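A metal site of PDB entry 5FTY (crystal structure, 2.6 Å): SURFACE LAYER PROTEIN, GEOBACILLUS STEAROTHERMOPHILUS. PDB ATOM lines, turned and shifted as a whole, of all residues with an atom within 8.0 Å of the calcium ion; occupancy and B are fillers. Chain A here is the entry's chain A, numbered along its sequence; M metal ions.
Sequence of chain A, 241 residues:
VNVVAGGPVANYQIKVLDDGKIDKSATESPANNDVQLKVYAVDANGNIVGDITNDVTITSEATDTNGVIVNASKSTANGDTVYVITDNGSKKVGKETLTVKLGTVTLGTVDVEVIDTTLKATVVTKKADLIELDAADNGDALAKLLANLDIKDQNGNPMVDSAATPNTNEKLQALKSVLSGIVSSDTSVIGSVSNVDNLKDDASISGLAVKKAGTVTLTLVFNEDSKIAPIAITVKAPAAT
The calcium ion is bound by O of Ser 25 (2.4 Å). OD1 of Asn 33 binds the calcium ion (2.4 Å). The calcium ion is bound by OE1 of Glu 28 (2.5 Å). The calcium ion is bound by O of Asp 23 (2.5 Å). The calcium ion is bound by OE2 of Glu 28 (2.5 Å).
OD1 of Asp 23 lies close to N of Ser 25, at 3.2 Å. The backbone NH (N) of Thr 27 lies within hydrogen-bond range of the side-chain hydroxyl (OG) of Ser 25 (3.3 Å). The side-chain hydroxyl (OG) of Ser 25 lies close to the side-chain hydroxyl (OG1) of Thr 118. OE2 of Glu 28 lies close to N of Asn 32 (2.8 Å). N of Asp 23 sits at hydrogen-bond distance from O of Asn 32 (2.6 Å). OD2 of Asp 23 lies within hydrogen-bond range of OG1 of Thr 117.
Of the 18 residues printed, 4 come within 4 Å of the calcium ion. The nearest printed residue that does not touch the calcium ion is Lys 24 (4.1 Å).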
ATOM      1  N   ILE A  22       7.633 -19.512  -3.284  1.00  0.00           N
ATOM      2  CA  ILE A  22       8.664 -19.655  -2.268  1.00  0.00           C
ATOM      3  C   ILE A  22       8.460 -20.979  -1.529  1.00  0.00           C
ATOM      4  O   ILE A  22       7.462 -21.161  -0.831  1.00  0.00           O
ATOM      5  CB  ILE A  22       8.616 -18.506  -1.244  1.00  0.00           C
ATOM      6  CG1 ILE A  22       8.939 -17.182  -1.923  1.00  0.00           C
ATOM      7  CG2 ILE A  22       9.584 -18.776  -0.101  1.00  0.00           C
ATOM      8  CD1 ILE A  22       8.672 -15.980  -1.048  1.00  0.00           C
ATOM      9  N   ASP A  23       9.409 -21.906  -1.690  1.00  0.00           N
ATOM     10  CA  ASP A  23       9.289 -23.198  -1.032  1.00  0.00           C
ATOM     11  C   ASP A  23       9.669 -23.115   0.444  1.00  0.00           C
ATOM     12  O   ASP A  23      10.786 -22.739   0.787  1.00  0.00           O
ATOM     13  CB  ASP A  23      10.152 -24.257  -1.743  1.00  0.00           C
ATOM     14  CG  ASP A  23       9.600 -25.666  -1.584  1.00  0.00           C
ATOM     15  OD1 ASP A  23       8.818 -25.893  -0.630  1.00  0.00           O
ATOM     16  OD2 ASP A  23       9.943 -26.538  -2.407  1.00  0.00           O
ATOM     17  N   LYS A  24       8.722 -23.466   1.303  1.00  0.00           N
ATOM     18  CA  LYS A  24       8.928 -23.417   2.736  1.00  0.00           C
ATOM     19  C   LYS A  24       9.724 -24.636   3.208  1.00  0.00           C
ATOM     20  O   LYS A  24      10.166 -24.689   4.357  1.00  0.00           O
ATOM     21  CB  LYS A  24       7.576 -23.335   3.456  1.00  0.00           C
ATOM     22  CG  LYS A  24       7.656 -22.929   4.919  1.00  0.00           C
ATOM     23  CD  LYS A  24       6.265 -22.807   5.515  1.00  0.00           C
ATOM     24  CE  LYS A  24       5.413 -24.020   5.184  1.00  0.00           C
ATOM     25  NZ  LYS A  24       4.058 -23.950   5.803  1.00  0.00           N
ATOM     26  N   SER A  25       9.910 -25.599   2.315  1.00  0.00           N
ATOM     27  CA  SER A  25      10.679 -26.800   2.618  1.00  0.00           C
ATOM     28  C   SER A  25      12.126 -26.460   2.943  1.00  0.00           C
ATOM     29  O   SER A  25      12.602 -25.353   2.670  1.00  0.00           O
ATOM     30  CB  SER A  25      10.626 -27.791   1.454  1.00  0.00           C
ATOM     31  OG  SER A  25      11.447 -28.922   1.708  1.00  0.00           O
ATOM     32  N   ALA A  26      12.839 -27.418   3.514  1.00  0.00           N
ATOM     33  CA  ALA A  26      14.227 -27.206   3.894  1.00  0.00           C
ATOM     34  C   ALA A  26      15.193 -27.915   2.939  1.00  0.00           C
ATOM     35  O   ALA A  26      16.384 -27.600   2.900  1.00  0.00           O
ATOM     36  CB  ALA A  26      14.463 -27.679   5.327  1.00  0.00           C
ATOM     37  N   THR A  27      14.667 -28.860   2.169  1.00  0.00           N
ATOM     38  CA  THR A  27      15.523 -29.714   1.345  1.00  0.00           C
ATOM     39  C   THR A  27      15.088 -29.833  -0.115  1.00  0.00           C
ATOM     40  O   THR A  27      15.303 -30.877  -0.732  1.00  0.00           O
ATOM     41  CB  THR A  27      15.628 -31.133   1.922  1.00  0.00           C
ATOM     42  OG1 THR A  27      14.323 -31.742   1.934  1.00  0.00           O
ATOM     43  CG2 THR A  27      16.190 -31.109   3.339  1.00  0.00           C
ATOM     44  N   GLU A  28      14.493 -28.792  -0.688  1.00  0.00           N
ATOM     45  CA  GLU A  28      14.081 -28.865  -2.086  1.00  0.00           C
ATOM     46  C   GLU A  28      15.244 -28.578  -3.032  1.00  0.00           C
ATOM     47  O   GLU A  28      16.124 -27.786  -2.727  1.00  0.00           O
ATOM     48  CB  GLU A  28      12.884 -27.951  -2.380  1.00  0.00           C
ATOM     49  CG  GLU A  28      13.250 -26.496  -2.673  1.00  0.00           C
ATOM     50  CD  GLU A  28      13.392 -25.663  -1.411  1.00  0.00           C
ATOM     51  OE1 GLU A  28      12.956 -26.138  -0.341  1.00  0.00           O
ATOM     52  OE2 GLU A  28      13.936 -24.546  -1.503  1.00  0.00           O
ATOM     53  N   SER A  29      15.238 -29.257  -4.183  1.00  0.00           N
ATOM     54  CA  SER A  29      16.278 -29.070  -5.186  1.00  0.00           C
ATOM     55  C   SER A  29      15.646 -28.910  -6.562  1.00  0.00           C
ATOM     56  O   SER A  29      14.921 -29.796  -7.017  1.00  0.00           O
ATOM     57  CB  SER A  29      17.247 -30.246  -5.167  1.00  0.00           C
ATOM     58  OG  SER A  29      18.393 -29.962  -5.951  1.00  0.00           O
ATOM     59  N   PRO A  30      15.918 -27.780  -7.242  1.00  0.00           N
ATOM     60  CA  PRO A  30      16.797 -26.687  -6.810  1.00  0.00           C
ATOM     61  C   PRO A  30      16.171 -25.841  -5.712  1.00  0.00           C
ATOM     62  O   PRO A  30      14.959 -25.887  -5.508  1.00  0.00           O
ATOM     63  CB  PRO A  30      16.949 -25.841  -8.079  1.00  0.00           C
ATOM     64  CG  PRO A  30      16.423 -26.676  -9.186  1.00  0.00           C
ATOM     65  CD  PRO A  30      15.371 -27.534  -8.578  1.00  0.00           C
ATOM     66  N   ALA A  31      17.005 -25.078  -4.997  1.00  0.00           N
ATOM     67  CA  ALA A  31      16.528 -24.198  -3.942  1.00  0.00           C
ATOM     68  C   ALA A  31      15.563 -23.152  -4.480  1.00  0.00           C
ATOM     69  O   ALA A  31      15.890 -22.400  -5.393  1.00  0.00           O
ATOM     70  CB  ALA A  31      17.705 -23.541  -3.239  1.00  0.00           C
ATOM     71  N   ASN A  32      14.355 -23.135  -3.920  1.00  0.00           N
ATOM     72  CA  ASN A  32      13.310 -22.229  -4.368  1.00  0.00           C
ATOM     73  C   ASN A  32      12.892 -21.301  -3.228  1.00  0.00           C
ATOM     74  O   ASN A  32      11.750 -21.332  -2.779  1.00  0.00           O
ATOM     75  CB  ASN A  32      12.108 -23.050  -4.848  1.00  0.00           C
ATOM     76  CG  ASN A  32      11.138 -22.227  -5.674  1.00  0.00           C
ATOM     77  OD1 ASN A  32      11.277 -21.016  -5.779  1.00  0.00           O
ATOM     78  ND2 ASN A  32      10.156 -22.889  -6.274  1.00  0.00           N
ATOM     79  N   ASN A  33      13.820 -20.460  -2.788  1.00  0.00           N
ATOM     80  CA  ASN A  33      13.641 -19.681  -1.559  1.00  0.00           C
ATOM     81  C   ASN A  33      13.271 -18.209  -1.710  1.00  0.00           C
ATOM     82  O   ASN A  33      13.298 -17.461  -0.729  1.00  0.00           O
ATOM     83  CB  ASN A  33      14.889 -19.806  -0.678  1.00  0.00           C
ATOM     84  CG  ASN A  33      15.052 -21.183  -0.066  1.00  0.00           C
ATOM     85  OD1 ASN A  33      14.070 -21.832   0.268  1.00  0.00           O
ATOM     86  ND2 ASN A  33      16.287 -21.610   0.098  1.00  0.00           N
ATOM     87  N   ASP A  34      12.939 -17.777  -2.928  1.00  0.00           N
ATOM     88  CA  ASP A  34      12.557 -16.381  -3.130  1.00  0.00           C
ATOM     89  C   ASP A  34      11.684 -16.140  -4.360  1.00  0.00           C
ATOM     90  O   ASP A  34      11.516 -17.016  -5.201  1.00  0.00           O
ATOM     91  CB  ASP A  34      13.791 -15.461  -3.172  1.00  0.00           C
ATOM     92  CG  ASP A  34      14.720 -15.782  -4.341  1.00  0.00           C
ATOM     93  OD1 ASP A  34      14.250 -15.904  -5.489  1.00  0.00           O
ATOM     94  OD2 ASP A  34      15.945 -15.896  -4.100  1.00  0.00           O
ATOM     95  N   ASP A  87      10.900 -15.649   2.765  1.00  0.00           N
ATOM     96  CA  ASP A  87      10.001 -16.131   3.817  1.00  0.00           C
ATOM     97  C   ASP A  87      10.333 -15.499   5.168  1.00  0.00           C
ATOM     98  O   ASP A  87      11.501 -15.344   5.523  1.00  0.00           O
ATOM     99  CB  ASP A  87      10.061 -17.661   3.926  1.00  0.00           C
ATOM    100  CG  ASP A  87       9.080 -18.217   4.946  1.00  0.00           C
ATOM    101  OD1 ASP A  87       8.123 -17.511   5.317  1.00  0.00           O
ATOM    102  OD2 ASP A  87       9.273 -19.378   5.383  1.00  0.00           O
ATOM    103  N   ILE A 115       4.743 -22.310  -0.867  1.00  0.00           N
ATOM    104  CA  ILE A 115       4.426 -23.725  -0.974  1.00  0.00           C
ATOM    105  C   ILE A 115       5.330 -24.553  -0.050  1.00  0.00           C
ATOM    106  O   ILE A 115       6.344 -24.061   0.431  1.00  0.00           O
ATOM    107  CB  ILE A 115       4.604 -24.243  -2.416  1.00  0.00           C
ATOM    108  CG1 ILE A 115       6.058 -24.115  -2.861  1.00  0.00           C
ATOM    109  CG2 ILE A 115       3.687 -23.495  -3.362  1.00  0.00           C
ATOM    110  CD1 ILE A 115       6.317 -24.672  -4.241  1.00  0.00           C
ATOM    111  N   ASP A 116       4.935 -25.797   0.187  1.00  0.00           N
ATOM    112  CA  ASP A 116       5.750 -26.703   0.979  1.00  0.00           C
ATOM    113  C   ASP A 116       5.780 -28.094   0.342  1.00  0.00           C
ATOM    114  O   ASP A 116       4.860 -28.888   0.540  1.00  0.00           O
ATOM    115  CB  ASP A 116       5.222 -26.786   2.418  1.00  0.00           C
ATOM    116  CG  ASP A 116       6.256 -27.304   3.393  1.00  0.00           C
ATOM    117  OD1 ASP A 116       7.235 -27.938   2.930  1.00  0.00           O
ATOM    118  OD2 ASP A 116       6.112 -27.075   4.610  1.00  0.00           O
ATOM    119  N   THR A 117       6.839 -28.372  -0.400  1.00  0.00           N
ATOM    120  CA  THR A 117       6.972 -29.648  -1.101  1.00  0.00           C
ATOM    121  C   THR A 117       7.716 -30.686  -0.268  1.00  0.00           C
ATOM    122  O   THR A 117       8.263 -31.654  -0.812  1.00  0.00           O
ATOM    123  CB  THR A 117       7.691 -29.483  -2.455  1.00  0.00           C
ATOM    124  OG1 THR A 117       9.060 -29.142  -2.238  1.00  0.00           O
ATOM    125  CG2 THR A 117       7.025 -28.391  -3.287  1.00  0.00           C
ATOM    126  N   THR A 118       7.754 -30.488   1.043  1.00  0.00           N
ATOM    127  CA  THR A 118       8.384 -31.430   1.962  1.00  0.00           C
ATOM    128  C   THR A 118       7.723 -32.794   1.868  1.00  0.00           C
ATOM    129  O   THR A 118       6.500 -32.886   1.732  1.00  0.00           O
ATOM    130  CB  THR A 118       8.313 -30.933   3.411  1.00  0.00           C
ATOM    131  OG1 THR A 118       8.744 -29.563   3.472  1.00  0.00           O
ATOM    132  CG2 THR A 118       9.199 -31.766   4.312  1.00  0.00           C
HETATM  133 CA    CA M   1      12.997 -23.950   0.771  1.00  0.00          CA
